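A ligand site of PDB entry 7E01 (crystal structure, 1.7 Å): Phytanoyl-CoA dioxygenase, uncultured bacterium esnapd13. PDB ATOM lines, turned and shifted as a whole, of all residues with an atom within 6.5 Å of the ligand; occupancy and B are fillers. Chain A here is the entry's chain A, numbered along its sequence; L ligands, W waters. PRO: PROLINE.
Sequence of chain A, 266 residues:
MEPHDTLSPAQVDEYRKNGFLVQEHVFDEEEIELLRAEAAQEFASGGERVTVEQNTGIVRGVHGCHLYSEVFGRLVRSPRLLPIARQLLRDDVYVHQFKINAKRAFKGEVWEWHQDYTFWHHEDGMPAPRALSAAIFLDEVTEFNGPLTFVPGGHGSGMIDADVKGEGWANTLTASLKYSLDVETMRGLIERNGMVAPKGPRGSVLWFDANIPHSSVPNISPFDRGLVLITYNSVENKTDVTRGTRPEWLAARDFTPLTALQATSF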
ATOM      1  N   HIS A  63      27.215   1.418 -18.497  1.00  0.00           N
ATOM      2  CA  HIS A  63      28.140   0.465 -19.165  1.00  0.00           C
ATOM      3  C   HIS A  63      29.339   1.109 -19.829  1.00  0.00           C
ATOM      4  O   HIS A  63      29.258   2.151 -20.460  1.00  0.00           O
ATOM      5  CB  HIS A  63      27.341  -0.356 -20.204  1.00  0.00           C
ATOM      6  CG  HIS A  63      26.162  -1.020 -19.587  1.00  0.00           C
ATOM      7  ND1 HIS A  63      25.027  -0.297 -19.215  1.00  0.00           N
ATOM      8  CD2 HIS A  63      25.981  -2.278 -19.136  1.00  0.00           C
ATOM      9  CE1 HIS A  63      24.193  -1.100 -18.597  1.00  0.00           C
ATOM     10  NE2 HIS A  63      24.742  -2.298 -18.521  1.00  0.00           N
ATOM     11  N   HIS A  96      36.232  -7.366 -21.133  1.00  0.00           N
ATOM     12  CA  HIS A  96      35.119  -7.563 -22.091  1.00  0.00           C
ATOM     13  C   HIS A  96      34.016  -6.570 -21.907  1.00  0.00           C
ATOM     14  O   HIS A  96      33.538  -6.015 -22.853  1.00  0.00           O
ATOM     15  CB  HIS A  96      34.614  -8.979 -21.890  1.00  0.00           C
ATOM     16  CG  HIS A  96      33.447  -9.297 -22.754  1.00  0.00           C
ATOM     17  ND1 HIS A  96      33.494  -9.180 -24.128  1.00  0.00           N
ATOM     18  CD2 HIS A  96      32.148  -9.558 -22.446  1.00  0.00           C
ATOM     19  CE1 HIS A  96      32.285  -9.315 -24.630  1.00  0.00           C
ATOM     20  NE2 HIS A  96      31.464  -9.654 -23.643  1.00  0.00           N
ATOM     21  N   GLN A  97      33.701  -6.349 -20.658  1.00  0.00           N
ATOM     22  CA  GLN A  97      32.521  -5.563 -20.220  1.00  0.00           C
ATOM     23  C   GLN A  97      32.712  -4.942 -18.856  1.00  0.00           C
ATOM     24  O   GLN A  97      33.343  -5.569 -17.989  1.00  0.00           O
ATOM     25  CB  GLN A  97      31.282  -6.523 -20.152  1.00  0.00           C
ATOM     26  CG  GLN A  97      29.948  -5.783 -19.841  1.00  0.00           C
ATOM     27  CD  GLN A  97      28.712  -6.724 -19.973  1.00  0.00           C
ATOM     28  OE1 GLN A  97      28.294  -7.460 -19.051  1.00  0.00           O
ATOM     29  NE2 GLN A  97      28.282  -6.860 -21.204  1.00  0.00           N
ATOM     30  N   LYS A  99      30.303  -2.705 -16.009  1.00  0.00           N
ATOM     31  CA  LYS A  99      28.969  -2.009 -15.771  1.00  0.00           C
ATOM     32  C   LYS A  99      28.905  -1.652 -14.322  1.00  0.00           C
ATOM     33  O   LYS A  99      29.489  -2.323 -13.455  1.00  0.00           O
ATOM     34  CB  LYS A  99      27.887  -2.970 -16.219  1.00  0.00           C
ATOM     35  CG  LYS A  99      27.855  -4.309 -15.597  1.00  0.00           C
ATOM     36  CD  LYS A  99      26.925  -5.316 -16.349  1.00  0.00           C
ATOM     37  CE  LYS A  99      26.981  -6.705 -15.703  1.00  0.00           C
ATOM     38  NZ  LYS A  99      28.152  -7.410 -16.352  1.00  0.00           N
ATOM     39  N   TRP A 111      15.730 -10.103 -10.529  1.00  0.00           N
ATOM     40  CA  TRP A 111      16.517 -10.349 -11.716  1.00  0.00           C
ATOM     41  C   TRP A 111      16.502 -11.778 -11.927  1.00  0.00           C
ATOM     42  O   TRP A 111      17.034 -12.577 -11.123  1.00  0.00           O
ATOM     43  CB  TRP A 111      17.952 -10.045 -11.585  1.00  0.00           C
ATOM     44  CG  TRP A 111      18.247  -8.619 -11.706  1.00  0.00           C
ATOM     45  CD1 TRP A 111      17.842  -7.627 -10.847  1.00  0.00           C
ATOM     46  CD2 TRP A 111      19.080  -7.979 -12.694  1.00  0.00           C
ATOM     47  NE1 TRP A 111      18.351  -6.431 -11.234  1.00  0.00           N
ATOM     48  CE2 TRP A 111      19.094  -6.576 -12.349  1.00  0.00           C
ATOM     49  CE3 TRP A 111      19.751  -8.400 -13.811  1.00  0.00           C
ATOM     50  CZ2 TRP A 111      19.784  -5.652 -13.088  1.00  0.00           C
ATOM     51  CZ3 TRP A 111      20.430  -7.458 -14.543  1.00  0.00           C
ATOM     52  CH2 TRP A 111      20.448  -6.123 -14.185  1.00  0.00           C
ATOM     53  N   HIS A 114      20.064 -16.518 -14.472  1.00  0.00           N
ATOM     54  CA  HIS A 114      20.737 -16.496 -15.791  1.00  0.00           C
ATOM     55  C   HIS A 114      22.254 -16.715 -15.614  1.00  0.00           C
ATOM     56  O   HIS A 114      22.762 -16.796 -14.456  1.00  0.00           O
ATOM     57  CB  HIS A 114      20.501 -15.217 -16.550  1.00  0.00           C
ATOM     58  CG  HIS A 114      21.182 -14.018 -15.943  1.00  0.00           C
ATOM     59  ND1 HIS A 114      20.846 -13.512 -14.706  1.00  0.00           N
ATOM     60  CD2 HIS A 114      22.170 -13.222 -16.438  1.00  0.00           C
ATOM     61  CE1 HIS A 114      21.604 -12.453 -14.465  1.00  0.00           C
ATOM     62  NE2 HIS A 114      22.420 -12.268 -15.484  1.00  0.00           N
ATOM     63  N   GLN A 115      22.882 -17.009 -16.762  1.00  0.00           N
ATOM     64  CA  GLN A 115      24.354 -17.290 -16.821  1.00  0.00           C
ATOM     65  C   GLN A 115      24.862 -16.203 -17.754  1.00  0.00           C
ATOM     66  O   GLN A 115      24.379 -16.042 -18.839  1.00  0.00           O
ATOM     67  CB  GLN A 115      24.728 -18.711 -17.338  1.00  0.00           C
ATOM     68  CG  GLN A 115      24.295 -19.866 -16.531  1.00  0.00           C
ATOM     69  CD  GLN A 115      24.513 -21.131 -17.346  1.00  0.00           C
ATOM     70  OE1 GLN A 115      23.880 -21.322 -18.440  1.00  0.00           O
ATOM     71  NE2 GLN A 115      25.354 -21.991 -16.848  1.00  0.00           N
ATOM     72  N   ASP A 116      25.887 -15.464 -17.272  1.00  0.00           N
ATOM     73  CA  ASP A 116      26.386 -14.392 -18.042  1.00  0.00           C
ATOM     74  C   ASP A 116      26.917 -14.831 -19.416  1.00  0.00           C
ATOM     75  O   ASP A 116      26.749 -14.077 -20.372  1.00  0.00           O
ATOM     76  CB  ASP A 116      27.547 -13.663 -17.272  1.00  0.00           C
ATOM     77  CG  ASP A 116      27.101 -12.859 -16.076  1.00  0.00           C
ATOM     78  OD1 ASP A 116      25.963 -12.380 -16.064  1.00  0.00           O
ATOM     79  OD2 ASP A 116      27.985 -12.570 -15.209  1.00  0.00           O
ATOM     80  N   TYR A 117      27.614 -16.006 -19.477  1.00  0.00           N
ATOM     81  CA  TYR A 117      28.306 -16.492 -20.713  1.00  0.00           C
ATOM     82  C   TYR A 117      27.321 -16.745 -21.898  1.00  0.00           C
ATOM     83  O   TYR A 117      27.601 -16.522 -23.045  1.00  0.00           O
ATOM     84  CB  TYR A 117      29.087 -17.734 -20.370  1.00  0.00           C
ATOM     85  CG  TYR A 117      29.680 -18.401 -21.570  1.00  0.00           C
ATOM     86  CD1 TYR A 117      30.618 -17.751 -22.364  1.00  0.00           C
ATOM     87  CD2 TYR A 117      29.251 -19.665 -21.986  1.00  0.00           C
ATOM     88  CE1 TYR A 117      31.147 -18.341 -23.517  1.00  0.00           C
ATOM     89  CE2 TYR A 117      29.759 -20.262 -23.139  1.00  0.00           C
ATOM     90  CZ  TYR A 117      30.726 -19.599 -23.907  1.00  0.00           C
ATOM     91  OH  TYR A 117      31.255 -20.233 -25.013  1.00  0.00           O
ATOM     92  N   PHE A 119      24.935 -14.767 -22.850  1.00  0.00           N
ATOM     93  CA  PHE A 119      24.852 -13.550 -23.578  1.00  0.00           C
ATOM     94  C   PHE A 119      26.115 -13.319 -24.350  1.00  0.00           C
ATOM     95  O   PHE A 119      26.128 -12.908 -25.478  1.00  0.00           O
ATOM     96  CB  PHE A 119      24.689 -12.339 -22.640  1.00  0.00           C
ATOM     97  CG  PHE A 119      23.410 -12.352 -21.805  1.00  0.00           C
ATOM     98  CD1 PHE A 119      23.265 -13.199 -20.726  1.00  0.00           C
ATOM     99  CD2 PHE A 119      22.404 -11.464 -22.121  1.00  0.00           C
ATOM    100  CE1 PHE A 119      22.089 -13.240 -19.974  1.00  0.00           C
ATOM    101  CE2 PHE A 119      21.242 -11.460 -21.383  1.00  0.00           C
ATOM    102  CZ  PHE A 119      21.087 -12.350 -20.306  1.00  0.00           C
ATOM    103  N   TRP A 120      27.245 -13.526 -23.707  1.00  0.00           N
ATOM    104  CA  TRP A 120      28.484 -13.154 -24.352  1.00  0.00           C
ATOM    105  C   TRP A 120      28.793 -14.069 -25.538  1.00  0.00           C
ATOM    106  O   TRP A 120      29.278 -13.646 -26.539  1.00  0.00           O
ATOM    107  CB  TRP A 120      29.612 -13.200 -23.293  1.00  0.00           C
ATOM    108  CG  TRP A 120      29.432 -12.188 -22.164  1.00  0.00           C
ATOM    109  CD1 TRP A 120      28.732 -11.033 -22.233  1.00  0.00           C
ATOM    110  CD2 TRP A 120      29.959 -12.271 -20.876  1.00  0.00           C
ATOM    111  NE1 TRP A 120      28.766 -10.435 -21.022  1.00  0.00           N
ATOM    112  CE2 TRP A 120      29.437 -11.182 -20.148  1.00  0.00           C
ATOM    113  CE3 TRP A 120      30.722 -13.224 -20.201  1.00  0.00           C
ATOM    114  CZ2 TRP A 120      29.762 -10.930 -18.838  1.00  0.00           C
ATOM    115  CZ3 TRP A 120      31.010 -13.017 -18.781  1.00  0.00           C
ATOM    116  CH2 TRP A 120      30.509 -11.850 -18.144  1.00  0.00           C
ATOM    117  N   GLU A 123      25.586 -13.171 -28.195  1.00  0.00           N
ATOM    118  CA  GLU A 123      25.547 -11.804 -28.660  1.00  0.00           C
ATOM    119  C   GLU A 123      26.910 -11.310 -29.119  1.00  0.00           C
ATOM    120  O   GLU A 123      27.037 -10.466 -29.976  1.00  0.00           O
ATOM    121  CB  GLU A 123      25.030 -10.859 -27.535  1.00  0.00           C
ATOM    122  CG  GLU A 123      23.679 -11.192 -26.866  1.00  0.00           C
ATOM    123  CD  GLU A 123      22.518 -11.063 -27.859  1.00  0.00           C
ATOM    124  OE1 GLU A 123      22.452  -9.966 -28.513  1.00  0.00           O
ATOM    125  OE2 GLU A 123      21.778 -12.074 -28.010  1.00  0.00           O
ATOM    126  N   ASP A 124      27.985 -11.816 -28.479  1.00  0.00           N
ATOM    127  CA  ASP A 124      29.292 -11.168 -28.715  1.00  0.00           C
ATOM    128  C   ASP A 124      30.328 -12.047 -29.423  1.00  0.00           C
ATOM    129  O   ASP A 124      31.386 -11.544 -29.806  1.00  0.00           O
ATOM    130  CB  ASP A 124      29.863 -10.739 -27.326  1.00  0.00           C
ATOM    131  CG  ASP A 124      29.011  -9.748 -26.581  1.00  0.00           C
ATOM    132  OD1 ASP A 124      28.294  -8.919 -27.212  1.00  0.00           O
ATOM    133  OD2 ASP A 124      29.068  -9.795 -25.304  1.00  0.00           O
ATOM    134  N   TRP A 169      19.411  -6.575 -28.905  1.00  0.00           N
ATOM    135  CA  TRP A 169      20.043  -6.676 -27.560  1.00  0.00           C
ATOM    136  C   TRP A 169      19.472  -5.764 -26.465  1.00  0.00           C
ATOM    137  O   TRP A 169      19.772  -6.027 -25.307  1.00  0.00           O
ATOM    138  CB  TRP A 169      21.554  -6.440 -27.675  1.00  0.00           C
ATOM    139  CG  TRP A 169      21.948  -5.155 -28.379  1.00  0.00           C
ATOM    140  CD1 TRP A 169      22.281  -4.991 -29.716  1.00  0.00           C
ATOM    141  CD2 TRP A 169      22.105  -3.839 -27.770  1.00  0.00           C
ATOM    142  NE1 TRP A 169      22.625  -3.670 -29.963  1.00  0.00           N
ATOM    143  CE2 TRP A 169      22.498  -2.945 -28.810  1.00  0.00           C
ATOM    144  CE3 TRP A 169      21.886  -3.332 -26.476  1.00  0.00           C
ATOM    145  CZ2 TRP A 169      22.752  -1.566 -28.565  1.00  0.00           C
ATOM    146  CZ3 TRP A 169      22.116  -1.980 -26.241  1.00  0.00           C
ATOM    147  CH2 TRP A 169      22.544  -1.105 -27.293  1.00  0.00           C
ATOM    148  N   THR A 172      18.925  -7.371 -23.030  1.00  0.00           N
ATOM    149  CA  THR A 172      20.084  -7.945 -22.315  1.00  0.00           C
ATOM    150  C   THR A 172      20.508  -7.229 -21.014  1.00  0.00           C
ATOM    151  O   THR A 172      21.336  -7.770 -20.213  1.00  0.00           O
ATOM    152  CB  THR A 172      21.341  -8.004 -23.263  1.00  0.00           C
ATOM    153  OG1 THR A 172      21.745  -6.665 -23.704  1.00  0.00           O
ATOM    154  CG2 THR A 172      21.063  -8.972 -24.483  1.00  0.00           C
ATOM    155  N   LEU A 173      20.019  -6.012 -20.833  1.00  0.00           N
ATOM    156  CA  LEU A 173      20.372  -5.129 -19.705  1.00  0.00           C
ATOM    157  C   LEU A 173      19.153  -4.874 -18.759  1.00  0.00           C
ATOM    158  O   LEU A 173      19.241  -4.112 -17.808  1.00  0.00           O
ATOM    159  CB  LEU A 173      20.882  -3.809 -20.270  1.00  0.00           C
ATOM    160  CG  LEU A 173      21.927  -3.885 -21.364  1.00  0.00           C
ATOM    161  CD1 LEU A 173      22.272  -2.495 -21.822  1.00  0.00           C
ATOM    162  CD2 LEU A 173      23.125  -4.600 -20.742  1.00  0.00           C
ATOM    163  N   THR A 174      18.044  -5.543 -19.015  1.00  0.00           N
ATOM    164  CA  THR A 174      16.819  -5.285 -18.285  1.00  0.00           C
ATOM    165  C   THR A 174      16.515  -6.528 -17.368  1.00  0.00           C
ATOM    166  O   THR A 174      17.020  -7.610 -17.582  1.00  0.00           O
ATOM    167  CB  THR A 174      15.729  -4.944 -19.328  1.00  0.00           C
ATOM    168  OG1 THR A 174      15.591  -6.035 -20.261  1.00  0.00           O
ATOM    169  CG2 THR A 174      16.142  -3.689 -20.129  1.00  0.00           C
ATOM    170  N   LEU A 177      15.095 -10.246 -19.059  1.00  0.00           N
ATOM    171  CA  LEU A 177      16.343 -10.646 -19.735  1.00  0.00           C
ATOM    172  C   LEU A 177      16.104 -11.559 -20.896  1.00  0.00           C
ATOM    173  O   LEU A 177      15.311 -12.501 -20.807  1.00  0.00           O
ATOM    174  CB  LEU A 177      17.266 -11.442 -18.794  1.00  0.00           C
ATOM    175  CG  LEU A 177      18.007 -10.674 -17.735  1.00  0.00           C
ATOM    176  CD1 LEU A 177      18.759 -11.634 -16.860  1.00  0.00           C
ATOM    177  CD2 LEU A 177      18.948  -9.694 -18.414  1.00  0.00           C
ATOM    178  N   HIS A 214      22.941 -17.054 -11.765  1.00  0.00           N
ATOM    179  CA  HIS A 214      22.608 -16.094 -10.739  1.00  0.00           C
ATOM    180  C   HIS A 214      21.401 -15.226 -10.971  1.00  0.00           C
ATOM    181  O   HIS A 214      20.988 -15.047 -12.050  1.00  0.00           O
ATOM    182  CB  HIS A 214      23.848 -15.220 -10.383  1.00  0.00           C
ATOM    183  CG  HIS A 214      24.264 -14.310 -11.463  1.00  0.00           C
ATOM    184  ND1 HIS A 214      24.979 -14.750 -12.543  1.00  0.00           N
ATOM    185  CD2 HIS A 214      24.105 -12.979 -11.631  1.00  0.00           C
ATOM    186  CE1 HIS A 214      25.170 -13.743 -13.370  1.00  0.00           C
ATOM    187  NE2 HIS A 214      24.671 -12.655 -12.828  1.00  0.00           N
ATOM    188  N   ARG A 246      27.025  -5.910 -30.780  1.00  0.00           N
ATOM    189  CA  ARG A 246      26.769  -4.884 -29.767  1.00  0.00           C
ATOM    190  C   ARG A 246      27.872  -3.841 -29.793  1.00  0.00           C
ATOM    191  O   ARG A 246      28.950  -4.058 -30.393  1.00  0.00           O
ATOM    192  CB  ARG A 246      26.538  -5.503 -28.406  1.00  0.00           C
ATOM    193  CG  ARG A 246      25.477  -6.586 -28.353  1.00  0.00           C
ATOM    194  CD  ARG A 246      24.984  -6.791 -26.940  1.00  0.00           C
ATOM    195  NE  ARG A 246      25.985  -7.484 -26.126  1.00  0.00           N
ATOM    196  CZ  ARG A 246      25.828  -7.835 -24.858  1.00  0.00           C
ATOM    197  NH1 ARG A 246      24.687  -7.541 -24.211  1.00  0.00           N
ATOM    198  NH2 ARG A 246      26.818  -8.493 -24.220  1.00  0.00           N
ATOM    199  N   LEU A 250      29.508  -2.261 -24.592  1.00  0.00           N
ATOM    200  CA  LEU A 250      29.034  -3.492 -24.065  1.00  0.00           C
ATOM    201  C   LEU A 250      29.948  -4.681 -24.259  1.00  0.00           C
ATOM    202  O   LEU A 250      29.919  -5.620 -23.462  1.00  0.00           O
ATOM    203  CB  LEU A 250      27.632  -3.923 -24.636  1.00  0.00           C
ATOM    204  CG  LEU A 250      26.407  -3.073 -24.192  1.00  0.00           C
ATOM    205  CD1 LEU A 250      25.088  -3.681 -24.725  1.00  0.00           C
ATOM    206  CD2 LEU A 250      26.329  -3.097 -22.672  1.00  0.00           C
HETATM  207  N   PRO L   1      23.655  -8.538 -18.859  1.00  0.00           N
HETATM  208  CA  PRO L   1      25.035  -8.811 -19.352  1.00  0.00           C
HETATM  209  C   PRO L   1      25.138  -8.723 -20.856  1.00  0.00           C
HETATM  210  O   PRO L   1      26.220  -8.823 -21.490  1.00  0.00           O
HETATM  211  CB  PRO L   1      25.286 -10.205 -18.873  1.00  0.00           C
HETATM  212  CG  PRO L   1      24.150 -10.631 -17.907  1.00  0.00           C
HETATM  213  CD  PRO L   1      23.093  -9.578 -18.117  1.00  0.00           C
HETATM  214  OXT PRO L   1      24.101  -8.526 -21.485  1.00  0.00           O
HETATM  215  O   HOH W   1      23.486  -6.637 -16.974  1.00  0.00           O
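An oxygen (O) of the ligand is in hydrogen-bond range of the side-chain amide nitrogen of Gln 97, at 2.9 Å.
NE1 of Trp 120 sits at hydrogen-bond distance from O of the ligand (3.0 Å).
A nitrogen (N) of the ligand is in hydrogen-bond range of the backbone carbonyl oxygen of Thr 172, at 2.8 Å.
The guanidinium group (NH2) of Arg 246 is in salt-bridge range of an oxygen (O) of the ligand (2.8 Å).
The side-chain carboxylate (OD2) of Asp 124 lies within salt-bridge range of the guanidinium group (NH2) of Arg 246 (2.8 Å).
NH1 of Arg 246 lies within hydrogen-bond range of OG1 of Thr 172 (3.1 Å).
The side-chain carboxylate (OD1) of Asp 116 sits close to a ring nitrogen (NE2) of His 214 (3.5 Å).
O of Trp 169 lies within hydrogen-bond range of OG1 of Thr 172 (2.6 Å).
NZ of Lys 99 is in hydrogen-bond range of OE1 of Gln 97 (2.7 Å).
The side-chain amide nitrogen (NE2) of Gln 97 is in hydrogen-bond range of the backbone carbonyl oxygen (O) of Leu 250 (3.1 Å).
The backbone NH (N) of His 214 lies within hydrogen-bond range of the backbone carbonyl oxygen (O) of His 114 (2.7 Å).
Residues that only touch the ligand: His 114 (3.4 Å), Asp 116 (3.1 Å) and Phe 119 (3.5 Å).
Hydrophobic or aromatic side chains that line the ligand: His 114, Phe 119 and Trp 120.
Within 4 Å of the ligand: Gln 97, His 114, Asp 116, Phe 119, Trp 120, Thr 172 and Arg 246.
The nearest printed residue that does not touch the ligand is Leu 173 (4.1 Å).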
